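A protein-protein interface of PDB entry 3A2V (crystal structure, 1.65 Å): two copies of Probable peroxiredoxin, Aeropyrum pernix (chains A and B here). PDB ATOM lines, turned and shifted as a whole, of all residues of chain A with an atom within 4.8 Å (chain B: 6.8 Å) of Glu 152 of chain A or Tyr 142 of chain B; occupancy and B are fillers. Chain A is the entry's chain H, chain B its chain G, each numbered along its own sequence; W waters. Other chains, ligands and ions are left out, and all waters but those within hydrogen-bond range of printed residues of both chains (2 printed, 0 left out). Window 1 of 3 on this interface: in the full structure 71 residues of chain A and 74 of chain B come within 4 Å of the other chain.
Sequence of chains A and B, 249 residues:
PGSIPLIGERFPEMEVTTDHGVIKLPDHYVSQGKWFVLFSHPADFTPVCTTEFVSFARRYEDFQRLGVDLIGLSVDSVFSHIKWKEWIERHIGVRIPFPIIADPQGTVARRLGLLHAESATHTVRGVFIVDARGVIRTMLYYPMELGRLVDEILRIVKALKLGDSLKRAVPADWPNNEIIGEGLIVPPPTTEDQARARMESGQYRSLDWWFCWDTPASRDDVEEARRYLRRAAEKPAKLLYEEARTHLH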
ATOM      1  N   ILE A   7      -8.712  15.069 -21.931  1.00  0.00           N
ATOM      2  CA  ILE A   7      -9.475  15.760 -20.892  1.00  0.00           C
ATOM      3  C   ILE A   7      -8.720  17.026 -20.472  1.00  0.00           C
ATOM      4  O   ILE A   7      -7.509  16.974 -20.239  1.00  0.00           O
ATOM      5  CB  ILE A   7      -9.711  14.858 -19.671  1.00  0.00           C
ATOM      6  CG1 ILE A   7     -10.607  13.658 -20.044  1.00  0.00           C
ATOM      7  CG2 ILE A   7     -10.337  15.651 -18.548  1.00  0.00           C
ATOM      8  CD1 ILE A   7     -10.698  12.573 -18.992  1.00  0.00           C
ATOM      9  N   THR A 138     -14.791  14.531 -20.061  1.00  0.00           N
ATOM     10  CA  THR A 138     -14.851  13.072 -19.892  1.00  0.00           C
ATOM     11  C   THR A 138     -14.901  12.499 -21.306  1.00  0.00           C
ATOM     12  O   THR A 138     -15.464  13.139 -22.197  1.00  0.00           O
ATOM     13  CB  THR A 138     -16.116  12.652 -19.091  1.00  0.00           C
ATOM     14  OG1 THR A 138     -15.964  13.063 -17.715  1.00  0.00           O
ATOM     15  CG2 THR A 138     -16.358  11.110 -19.123  1.00  0.00           C
ATOM     16  N   LEU A 140     -15.626   8.611 -23.282  1.00  0.00           N
ATOM     17  CA  LEU A 140     -15.892   7.175 -23.179  1.00  0.00           C
ATOM     18  C   LEU A 140     -15.723   6.529 -24.542  1.00  0.00           C
ATOM     19  O   LEU A 140     -16.093   7.132 -25.540  1.00  0.00           O
ATOM     20  CB  LEU A 140     -17.324   6.926 -22.703  1.00  0.00           C
ATOM     21  CG  LEU A 140     -17.783   7.838 -21.554  1.00  0.00           C
ATOM     22  CD1 LEU A 140     -19.257   7.698 -21.299  1.00  0.00           C
ATOM     23  CD2 LEU A 140     -16.999   7.437 -20.307  1.00  0.00           C
ATOM     24  N   LEU A 149     -24.843   2.941 -21.881  1.00  0.00           N
ATOM     25  CA  LEU A 149     -25.850   3.157 -20.841  1.00  0.00           C
ATOM     26  C   LEU A 149     -26.049   4.677 -20.792  1.00  0.00           C
ATOM     27  O   LEU A 149     -25.241   5.414 -20.206  1.00  0.00           O
ATOM     28  CB  LEU A 149     -25.321   2.655 -19.487  1.00  0.00           C
ATOM     29  CG  LEU A 149     -26.372   2.704 -18.364  1.00  0.00           C
ATOM     30  CD1 LEU A 149     -27.390   1.534 -18.566  1.00  0.00           C
ATOM     31  CD2 LEU A 149     -25.656   2.576 -17.011  1.00  0.00           C
ATOM     32  N   VAL A 150     -27.106   5.165 -21.422  1.00  0.00           N
ATOM     33  CA  VAL A 150     -27.262   6.593 -21.593  1.00  0.00           C
ATOM     34  C   VAL A 150     -27.504   7.347 -20.283  1.00  0.00           C
ATOM     35  O   VAL A 150     -27.085   8.487 -20.145  1.00  0.00           O
ATOM     36  CB  VAL A 150     -28.314   6.947 -22.681  1.00  0.00           C
ATOM     37  CG1 VAL A 150     -28.404   8.458 -22.862  1.00  0.00           C
ATOM     38  CG2 VAL A 150     -27.894   6.312 -23.987  1.00  0.00           C
ATOM     39  N   ASP A 151     -28.120   6.684 -19.298  1.00  0.00           N
ATOM     40  CA  ASP A 151     -28.332   7.325 -17.987  1.00  0.00           C
ATOM     41  C   ASP A 151     -27.009   7.642 -17.261  1.00  0.00           C
ATOM     42  O   ASP A 151     -26.973   8.598 -16.478  1.00  0.00           O
ATOM     43  CB  ASP A 151     -29.242   6.483 -17.114  1.00  0.00           C
ATOM     44  CG  ASP A 151     -30.672   6.443 -17.661  1.00  0.00           C
ATOM     45  OD1 ASP A 151     -31.243   7.531 -17.864  1.00  0.00           O
ATOM     46  OD2 ASP A 151     -31.196   5.336 -17.906  1.00  0.00           O
ATOM     47  N   GLU A 152     -25.944   6.883 -17.526  1.00  0.00           N
ATOM     48  CA  GLU A 152     -24.634   7.239 -16.918  1.00  0.00           C
ATOM     49  C   GLU A 152     -24.086   8.526 -17.571  1.00  0.00           C
ATOM     50  O   GLU A 152     -23.392   9.304 -16.933  1.00  0.00           O
ATOM     51  CB  GLU A 152     -23.640   6.074 -17.017  1.00  0.00           C
ATOM     52  CG  GLU A 152     -22.155   6.437 -16.716  1.00  0.00           C
ATOM     53  CD  GLU A 152     -21.944   6.969 -15.289  1.00  0.00           C
ATOM     54  OE1 GLU A 152     -22.927   7.031 -14.523  1.00  0.00           O
ATOM     55  OE2 GLU A 152     -20.788   7.280 -14.922  1.00  0.00           O
ATOM     56  N   ILE A 153     -24.401   8.766 -18.844  1.00  0.00           N
ATOM     57  CA  ILE A 153     -23.983  10.016 -19.475  1.00  0.00           C
ATOM     58  C   ILE A 153     -24.699  11.199 -18.798  1.00  0.00           C
ATOM     59  O   ILE A 153     -24.088  12.236 -18.555  1.00  0.00           O
ATOM     60  CB  ILE A 153     -24.220  10.002 -20.993  1.00  0.00           C
ATOM     61  CG1 ILE A 153     -23.436   8.827 -21.625  1.00  0.00           C
ATOM     62  CG2 ILE A 153     -23.867  11.383 -21.625  1.00  0.00           C
ATOM     63  CD1 ILE A 153     -23.720   8.666 -23.132  1.00  0.00           C
ATOM     64  N   LEU A 154     -25.983  11.014 -18.462  1.00  0.00           N
ATOM     65  CA  LEU A 154     -26.736  12.025 -17.703  1.00  0.00           C
ATOM     66  C   LEU A 154     -26.117  12.223 -16.319  1.00  0.00           C
ATOM     67  O   LEU A 154     -25.912  13.378 -15.885  1.00  0.00           O
ATOM     68  CB  LEU A 154     -28.207  11.631 -17.565  1.00  0.00           C
ATOM     69  CG  LEU A 154     -29.059  12.070 -18.772  1.00  0.00           C
ATOM     70  CD1 LEU A 154     -30.386  11.311 -18.707  1.00  0.00           C
ATOM     71  CD2 LEU A 154     -29.287  13.571 -18.761  1.00  0.00           C
ATOM     72  N   ARG A 155     -25.796  11.115 -15.652  1.00  0.00           N
ATOM     73  CA  ARG A 155     -25.210  11.199 -14.308  1.00  0.00           C
ATOM     74  C   ARG A 155     -23.886  11.941 -14.376  1.00  0.00           C
ATOM     75  O   ARG A 155     -23.607  12.791 -13.525  1.00  0.00           O
ATOM     76  CB  ARG A 155     -25.018   9.815 -13.671  1.00  0.00           C
ATOM     77  CG  ARG A 155     -24.645   9.890 -12.157  1.00  0.00           C
ATOM     78  CD  ARG A 155     -24.079   8.502 -11.687  1.00  0.00           C
ATOM     79  NE  ARG A 155     -22.733   8.269 -12.229  1.00  0.00           N
ATOM     80  CZ  ARG A 155     -21.606   8.646 -11.617  1.00  0.00           C
ATOM     81  NH1 ARG A 155     -21.655   9.250 -10.424  1.00  0.00           N
ATOM     82  NH2 ARG A 155     -20.435   8.447 -12.205  1.00  0.00           N
ATOM     83  N   ILE A 156     -23.065  11.623 -15.377  1.00  0.00           N
ATOM     84  CA  ILE A 156     -21.766  12.325 -15.537  1.00  0.00           C
ATOM     85  C   ILE A 156     -21.966  13.854 -15.658  1.00  0.00           C
ATOM     86  O   ILE A 156     -21.375  14.642 -14.896  1.00  0.00           O
ATOM     87  CB  ILE A 156     -20.964  11.742 -16.747  1.00  0.00           C
ATOM     88  CG1 ILE A 156     -20.443  10.351 -16.423  1.00  0.00           C
ATOM     89  CG2 ILE A 156     -19.820  12.697 -17.198  1.00  0.00           C
ATOM     90  CD1 ILE A 156     -20.009   9.532 -17.680  1.00  0.00           C
ATOM     91  N   GLU B  52     -13.359   5.049  -4.771  1.00  0.00           N
ATOM     92  CA  GLU B  52     -13.384   4.073  -5.901  1.00  0.00           C
ATOM     93  C   GLU B  52     -12.745   2.746  -5.531  1.00  0.00           C
ATOM     94  O   GLU B  52     -13.216   1.680  -5.945  1.00  0.00           O
ATOM     95  CB  GLU B  52     -12.695   4.643  -7.129  1.00  0.00           C
ATOM     96  CG  GLU B  52     -13.381   5.859  -7.703  1.00  0.00           C
ATOM     97  CD  GLU B  52     -12.665   6.414  -8.914  1.00  0.00           C
ATOM     98  OE1 GLU B  52     -11.436   6.639  -8.827  1.00  0.00           O
ATOM     99  OE2 GLU B  52     -13.327   6.661  -9.961  1.00  0.00           O
ATOM    100  N   GLU B 118      -5.323  17.823 -17.736  1.00  0.00           N
ATOM    101  CA  GLU B 118      -5.737  18.204 -16.380  1.00  0.00           C
ATOM    102  C   GLU B 118      -4.563  18.251 -15.409  1.00  0.00           C
ATOM    103  O   GLU B 118      -4.567  19.031 -14.445  1.00  0.00           O
ATOM    104  CB  GLU B 118      -6.752  17.202 -15.839  1.00  0.00           C
ATOM    105  CG  GLU B 118      -8.198  17.460 -16.235  1.00  0.00           C
ATOM    106  CD  GLU B 118      -9.161  16.749 -15.299  1.00  0.00           C
ATOM    107  OE1 GLU B 118     -10.079  17.443 -14.799  1.00  0.00           O
ATOM    108  OE2 GLU B 118      -8.972  15.511 -15.057  1.00  0.00           O
ATOM    109  N   THR B 123      -2.194  10.673 -13.294  1.00  0.00           N
ATOM    110  CA  THR B 123      -2.955   9.957 -14.290  1.00  0.00           C
ATOM    111  C   THR B 123      -4.443  10.347 -14.160  1.00  0.00           C
ATOM    112  O   THR B 123      -4.897  10.724 -13.074  1.00  0.00           O
ATOM    113  CB  THR B 123      -2.675   8.483 -13.925  1.00  0.00           C
ATOM    114  OG1 THR B 123      -2.114   7.734 -15.004  1.00  0.00           O
ATOM    115  CG2 THR B 123      -3.766   7.823 -13.173  1.00  0.00           C
ATOM    116  N   VAL B 124      -5.199  10.322 -15.268  1.00  0.00           N
ATOM    117  CA  VAL B 124      -6.665  10.479 -15.178  1.00  0.00           C
ATOM    118  C   VAL B 124      -7.268   9.211 -14.575  1.00  0.00           C
ATOM    119  O   VAL B 124      -6.537   8.303 -14.163  1.00  0.00           O
ATOM    120  CB  VAL B 124      -7.333  10.785 -16.581  1.00  0.00           C
ATOM    121  CG1 VAL B 124      -6.967  12.199 -17.048  1.00  0.00           C
ATOM    122  CG2 VAL B 124      -6.957   9.737 -17.608  1.00  0.00           C
ATOM    123  N   ARG B 125      -8.602   9.133 -14.557  1.00  0.00           N
ATOM    124  CA  ARG B 125      -9.266   7.940 -14.067  1.00  0.00           C
ATOM    125  C   ARG B 125      -9.620   7.082 -15.273  1.00  0.00           C
ATOM    126  O   ARG B 125     -10.772   7.085 -15.711  1.00  0.00           O
ATOM    127  CB  ARG B 125     -10.537   8.317 -13.294  1.00  0.00           C
ATOM    128  CG  ARG B 125     -10.238   9.243 -12.086  1.00  0.00           C
ATOM    129  CD  ARG B 125     -11.479   9.489 -11.207  1.00  0.00           C
ATOM    130  NE  ARG B 125     -11.076  10.537 -10.271  1.00  0.00           N
ATOM    131  CZ  ARG B 125     -10.363  10.290  -9.170  1.00  0.00           C
ATOM    132  NH1 ARG B 125      -9.917  11.307  -8.434  1.00  0.00           N
ATOM    133  NH2 ARG B 125     -10.082   9.025  -8.815  1.00  0.00           N
ATOM    134  N   GLY B 126      -8.632   6.343 -15.770  1.00  0.00           N
ATOM    135  CA  GLY B 126      -8.799   5.534 -16.976  1.00  0.00           C
ATOM    136  C   GLY B 126      -9.291   4.139 -16.633  1.00  0.00           C
ATOM    137  O   GLY B 126      -9.074   3.643 -15.521  1.00  0.00           O
ATOM    138  N   VAL B 127      -9.977   3.499 -17.590  1.00  0.00           N
ATOM    139  CA  VAL B 127     -10.472   2.143 -17.409  1.00  0.00           C
ATOM    140  C   VAL B 127     -10.208   1.409 -18.718  1.00  0.00           C
ATOM    141  O   VAL B 127     -10.632   1.874 -19.768  1.00  0.00           O
ATOM    142  CB  VAL B 127     -11.994   2.048 -17.055  1.00  0.00           C
ATOM    143  CG1 VAL B 127     -12.390   0.570 -16.870  1.00  0.00           C
ATOM    144  CG2 VAL B 127     -12.378   2.882 -15.807  1.00  0.00           C
ATOM    145  N   LEU B 140     -12.565   3.817 -20.881  1.00  0.00           N
ATOM    146  CA  LEU B 140     -13.306   4.945 -20.304  1.00  0.00           C
ATOM    147  C   LEU B 140     -12.268   5.910 -19.712  1.00  0.00           C
ATOM    148  O   LEU B 140     -11.306   5.459 -19.105  1.00  0.00           O
ATOM    149  CB  LEU B 140     -14.227   4.461 -19.185  1.00  0.00           C
ATOM    150  CG  LEU B 140     -15.115   3.234 -19.441  1.00  0.00           C
ATOM    151  CD1 LEU B 140     -15.854   2.878 -18.186  1.00  0.00           C
ATOM    152  CD2 LEU B 140     -16.077   3.544 -20.611  1.00  0.00           C
ATOM    153  N   TYR B 141     -12.469   7.209 -19.904  1.00  0.00           N
ATOM    154  CA  TYR B 141     -11.581   8.214 -19.276  1.00  0.00           C
ATOM    155  C   TYR B 141     -12.412   9.238 -18.493  1.00  0.00           C
ATOM    156  O   TYR B 141     -13.042  10.138 -19.064  1.00  0.00           O
ATOM    157  CB  TYR B 141     -10.703   8.926 -20.319  1.00  0.00           C
ATOM    158  CG  TYR B 141      -9.789   7.999 -21.101  1.00  0.00           C
ATOM    159  CD1 TYR B 141     -10.201   7.448 -22.310  1.00  0.00           C
ATOM    160  CD2 TYR B 141      -8.506   7.709 -20.640  1.00  0.00           C
ATOM    161  CE1 TYR B 141      -9.351   6.598 -23.041  1.00  0.00           C
ATOM    162  CE2 TYR B 141      -7.646   6.841 -21.354  1.00  0.00           C
ATOM    163  CZ  TYR B 141      -8.092   6.301 -22.556  1.00  0.00           C
ATOM    164  OH  TYR B 141      -7.252   5.453 -23.274  1.00  0.00           O
ATOM    165  N   TYR B 142     -12.422   9.049 -17.176  1.00  0.00           N
ATOM    166  CA  TYR B 142     -13.087   9.962 -16.251  1.00  0.00           C
ATOM    167  C   TYR B 142     -12.009  10.887 -15.737  1.00  0.00           C
ATOM    168  O   TYR B 142     -10.810  10.540 -15.752  1.00  0.00           O
ATOM    169  CB  TYR B 142     -13.759   9.231 -15.078  1.00  0.00           C
ATOM    170  CG  TYR B 142     -15.076   8.541 -15.411  1.00  0.00           C
ATOM    171  CD1 TYR B 142     -15.119   7.487 -16.335  1.00  0.00           C
ATOM    172  CD2 TYR B 142     -16.265   8.905 -14.763  1.00  0.00           C
ATOM    173  CE1 TYR B 142     -16.325   6.823 -16.623  1.00  0.00           C
ATOM    174  CE2 TYR B 142     -17.485   8.234 -15.049  1.00  0.00           C
ATOM    175  CZ  TYR B 142     -17.494   7.197 -15.980  1.00  0.00           C
ATOM    176  OH  TYR B 142     -18.685   6.516 -16.258  1.00  0.00           O
ATOM    177  N   PRO B 143     -12.431  12.073 -15.297  1.00  0.00           N
ATOM    178  CA  PRO B 143     -11.495  13.099 -14.829  1.00  0.00           C
ATOM    179  C   PRO B 143     -11.252  13.013 -13.329  1.00  0.00           C
ATOM    180  O   PRO B 143     -11.944  12.296 -12.607  1.00  0.00           O
ATOM    181  CB  PRO B 143     -12.259  14.369 -15.165  1.00  0.00           C
ATOM    182  CG  PRO B 143     -13.709  14.007 -14.845  1.00  0.00           C
ATOM    183  CD  PRO B 143     -13.829  12.533 -15.241  1.00  0.00           C
ATOM    184  N   MET B 144     -10.293  13.797 -12.840  1.00  0.00           N
ATOM    185  CA  MET B 144      -9.965  13.695 -11.424  1.00  0.00           C
ATOM    186  C   MET B 144     -11.118  14.060 -10.484  1.00  0.00           C
ATOM    187  O   MET B 144     -11.202  13.494  -9.396  1.00  0.00           O
ATOM    188  CB  MET B 144      -8.708  14.491 -11.073  1.00  0.00           C
ATOM    189  CG  MET B 144      -8.749  15.953 -11.424  1.00  0.00           C
ATOM    190  SD  MET B 144      -7.326  16.747 -10.683  1.00  0.00           S
ATOM    191  CE  MET B 144      -5.984  15.757 -11.367  1.00  0.00           C
ATOM    192  N   GLU B 145     -12.020  14.958 -10.902  1.00  0.00           N
ATOM    193  CA  GLU B 145     -13.061  15.472 -10.011  1.00  0.00           C
ATOM    194  C   GLU B 145     -14.335  14.598  -9.944  1.00  0.00           C
ATOM    195  O   GLU B 145     -15.293  14.916  -9.243  1.00  0.00           O
ATOM    196  CB  GLU B 145     -13.417  16.930 -10.379  1.00  0.00           C
ATOM    197  CG  GLU B 145     -14.117  17.138 -11.755  1.00  0.00           C
ATOM    198  CD  GLU B 145     -13.195  17.215 -12.956  1.00  0.00           C
ATOM    199  OE1 GLU B 145     -13.657  17.684 -14.022  1.00  0.00           O
ATOM    200  OE2 GLU B 145     -12.012  16.827 -12.889  1.00  0.00           O
ATOM    201  N   LEU B 146     -14.336  13.498 -10.695  1.00  0.00           N
ATOM    202  CA  LEU B 146     -15.566  12.713 -10.860  1.00  0.00           C
ATOM    203  C   LEU B 146     -15.290  11.224 -10.711  1.00  0.00           C
ATOM    204  O   LEU B 146     -14.620  10.619 -11.554  1.00  0.00           O
ATOM    205  CB  LEU B 146     -16.197  12.995 -12.229  1.00  0.00           C
ATOM    206  CG  LEU B 146     -17.461  12.140 -12.479  1.00  0.00           C
ATOM    207  CD1 LEU B 146     -18.656  12.583 -11.586  1.00  0.00           C
ATOM    208  CD2 LEU B 146     -17.884  12.204 -13.953  1.00  0.00           C
ATOM    209  N   GLY B 147     -15.826  10.627  -9.657  1.00  0.00           N
ATOM    210  CA  GLY B 147     -15.658   9.176  -9.440  1.00  0.00           C
ATOM    211  C   GLY B 147     -16.458   8.369 -10.466  1.00  0.00           C
ATOM    212  O   GLY B 147     -17.474   8.828 -10.990  1.00  0.00           O
ATOM    213  N   ARG B 148     -15.968   7.173 -10.739  1.00  0.00           N
ATOM    214  CA  ARG B 148     -16.619   6.265 -11.670  1.00  0.00           C
ATOM    215  C   ARG B 148     -17.883   5.628 -11.086  1.00  0.00           C
ATOM    216  O   ARG B 148     -18.120   5.661  -9.874  1.00  0.00           O
ATOM    217  CB  ARG B 148     -15.576   5.227 -12.135  1.00  0.00           C
ATOM    218  CG  ARG B 148     -14.577   5.846 -13.163  1.00  0.00           C
ATOM    219  CD  ARG B 148     -13.283   5.032 -13.313  1.00  0.00           C
ATOM    220  NE  ARG B 148     -12.400   5.280 -12.161  1.00  0.00           N
ATOM    221  CZ  ARG B 148     -11.085   5.087 -12.151  1.00  0.00           C
ATOM    222  NH1 ARG B 148     -10.440   4.620 -13.215  1.00  0.00           N
ATOM    223  NH2 ARG B 148     -10.393   5.368 -11.048  1.00  0.00           N
ATOM    224  N   LEU B 149     -18.728   5.078 -11.960  1.00  0.00           N
ATOM    225  CA  LEU B 149     -19.874   4.265 -11.531  1.00  0.00           C
ATOM    226  C   LEU B 149     -19.448   2.827 -11.765  1.00  0.00           C
ATOM    227  O   LEU B 149     -19.444   2.351 -12.896  1.00  0.00           O
ATOM    228  CB  LEU B 149     -21.105   4.586 -12.393  1.00  0.00           C
ATOM    229  CG  LEU B 149     -22.394   3.887 -11.959  1.00  0.00           C
ATOM    230  CD1 LEU B 149     -22.920   4.571 -10.658  1.00  0.00           C
ATOM    231  CD2 LEU B 149     -23.447   3.984 -13.080  1.00  0.00           C
ATOM    232  N   GLU B 152     -21.461   0.162 -13.703  1.00  0.00           N
ATOM    233  CA  GLU B 152     -21.424   0.186 -15.192  1.00  0.00           C
ATOM    234  C   GLU B 152     -20.235  -0.617 -15.749  1.00  0.00           C
ATOM    235  O   GLU B 152     -20.317  -1.222 -16.823  1.00  0.00           O
ATOM    236  CB  GLU B 152     -21.458   1.606 -15.765  1.00  0.00           C
ATOM    237  CG  GLU B 152     -21.250   1.692 -17.309  1.00  0.00           C
ATOM    238  CD  GLU B 152     -22.279   0.884 -18.142  1.00  0.00           C
ATOM    239  OE1 GLU B 152     -23.178   0.232 -17.557  1.00  0.00           O
ATOM    240  OE2 GLU B 152     -22.174   0.932 -19.388  1.00  0.00           O
ATOM    241  N   ILE B 153     -19.129  -0.662 -15.002  1.00  0.00           N
ATOM    242  CA  ILE B 153     -17.972  -1.428 -15.443  1.00  0.00           C
ATOM    243  C   ILE B 153     -18.297  -2.908 -15.381  1.00  0.00           C
ATOM    244  O   ILE B 153     -17.941  -3.650 -16.271  1.00  0.00           O
ATOM    245  CB  ILE B 153     -16.719  -1.075 -14.617  1.00  0.00           C
ATOM    246  CG1 ILE B 153     -16.430   0.412 -14.782  1.00  0.00           C
ATOM    247  CG2 ILE B 153     -15.568  -1.973 -15.007  1.00  0.00           C
ATOM    248  CD1 ILE B 153     -15.218   0.946 -13.913  1.00  0.00           C
ATOM    249  N   ASP B 173     -28.538   0.323 -23.068  1.00  0.00           N
ATOM    250  CA  ASP B 173     -29.237   0.137 -21.761  1.00  0.00           C
ATOM    251  C   ASP B 173     -29.620  -1.306 -21.418  1.00  0.00           C
ATOM    252  O   ASP B 173     -30.443  -1.534 -20.495  1.00  0.00           O
ATOM    253  CB  ASP B 173     -30.456   1.064 -21.675  1.00  0.00           C
ATOM    254  CG  ASP B 173     -30.150   2.479 -22.238  1.00  0.00           C
ATOM    255  OD1 ASP B 173     -29.197   3.135 -21.751  1.00  0.00           O
ATOM    256  OD2 ASP B 173     -30.875   2.903 -23.156  1.00  0.00           O
HETATM  257  O   HOH W   1     -19.176  10.024  -9.307  1.00  0.00           O
HETATM  258  O   HOH W   2     -29.273   3.965 -19.205  1.00  0.00           O
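Ile 7 of chain A touches Tyr 141 of chain B.
Tyr 142 of chain B touches Ile 7 of chain A (O to CD1, 3.8 Å).
Thr 138 of chain A touches Pro 143 of chain B.
Tyr 142 of chain B touches Leu 140 of chain A.
Leu 149 of chain A touches Glu 152 of chain B.
Leu 149 of chain A touches Asp 173 of chain B (CA to OD1, 3.5 Å).
CD2 of Leu 149 of chain B touches OE1 of Glu 152 of chain A (3.4 Å).
NH2 of Arg 155 of chain A touches C of Arg 148 of chain B (3.96 Å).
Leu 149 of chain B touches Arg 155 of chain A.
Tyr 142 of chain B touches Ile 156 of chain A.
The guanidinium group (NH1) of Arg 148 of chain B sits at hydrogen-bond distance from the backbone carbonyl oxygen (O) of Gly 126 of chain B (2.9 Å).
The guanidinium group (NE) of Arg 125 of chain B lies within hydrogen-bond range of the backbone carbonyl oxygen (O) of Pro 143 of chain B (3.1 Å).
The guanidinium group of Arg 148 of chain B lies within salt-bridge range of the side-chain carboxylate of Glu 52 of chain B (2.8 Å).
O of Tyr 142 of chain B is in hydrogen-bond range of N of Arg 125 of chain B, at 2.9 Å.
OE1 of Glu 152 of chain A is in salt-bridge range of NE of Arg 155 of chain A (2.6 Å).
OE2 of Glu 118 of chain B sits at hydrogen-bond distance from N of Met 144 of chain B, 3.1 Å away.
Leu 149 of chain A touches Glu 152 of chain B, and with the chains exchanged Glu 152 of chain A touches Leu 149 of chain B.
Of the 16 pairs that touch across the chains among the printed residues, 2 have their exchanged pair printed and touching as well.
Of the 20 printed residues of chain B, 10 touch a printed residue of chain A.
Hydrophobic or aromatic side chains of chain B that line the printed part of chain A: Tyr 141, Tyr 142, Pro 143, Leu 146 and Leu 149.
Hydrophobic or aromatic side chains of chain A within 4 Å of the printed part of chain B: Ile 7, Leu 140, Leu 149 and Ile 156.
Among the printed residues, 16 pairs touch across the chains.
The side-chain hydroxyl (OH) of Tyr 142 of chain B sits at hydrogen-bond distance from the side-chain carboxylate (OE2) of Glu 152 of chain A, at 2.6 Å.
The backbone NH (N) of Glu 118 of chain B is in hydrogen-bond range of the backbone carbonyl oxygen (O) of Ile 7 of chain A, 3.4 Å away.
O of Gly 147 of chain B sits at hydrogen-bond distance from NH2 of Arg 155 of chain A, 3.2 Å away.
The backbone NH (N) of Val 150 of chain A is in hydrogen-bond range of the side-chain carboxylate (OD1) of Asp 173 of chain B (2.9 Å).
Glu 152 of chain A touches two residues of chain B.
Printed residues of chain A within 4 Å of Tyr 142 of chain B: Ile 7 (3.8 Å), Leu 140 (3.8 Å), Glu 152 (2.6 Å) and Ile 156 (3.6 Å).
Printed residues of chain A within 4 Å of Asp 173 of chain B: Leu 149 and Val 150.
Of the printed residues of chain B, Val 150 of chain A touches Asp 173 (2.9 Å).
Printed residues of chain A within 4 Å of Leu 146 of chain B: Ile 156 (3.8 Å).
Of the printed residues of chain B, Leu 140 of chain A touches Tyr 142 (3.8 Å).
Printed residues of chain B within 4 Å of Thr 138 of chain A: Tyr 141 and Pro 143.
Val 124 of chain B touches none of the printed residues of chain A.
The nearest residue of chain A that does not touch Tyr 142 of chain B is Arg 155 of chain A (4.1 Å).
Water W1 lies within hydrogen-bond range of O of Gly 147 of chain B and NH1 of Arg 155 of chain A.
Water W2 lies within hydrogen-bond range of OD1 of Asp 173 of chain B (2.7 Å), OD2 of Asp 151 of chain A (2.7 Å) and N of Val 150 of chain A (3.3 Å).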
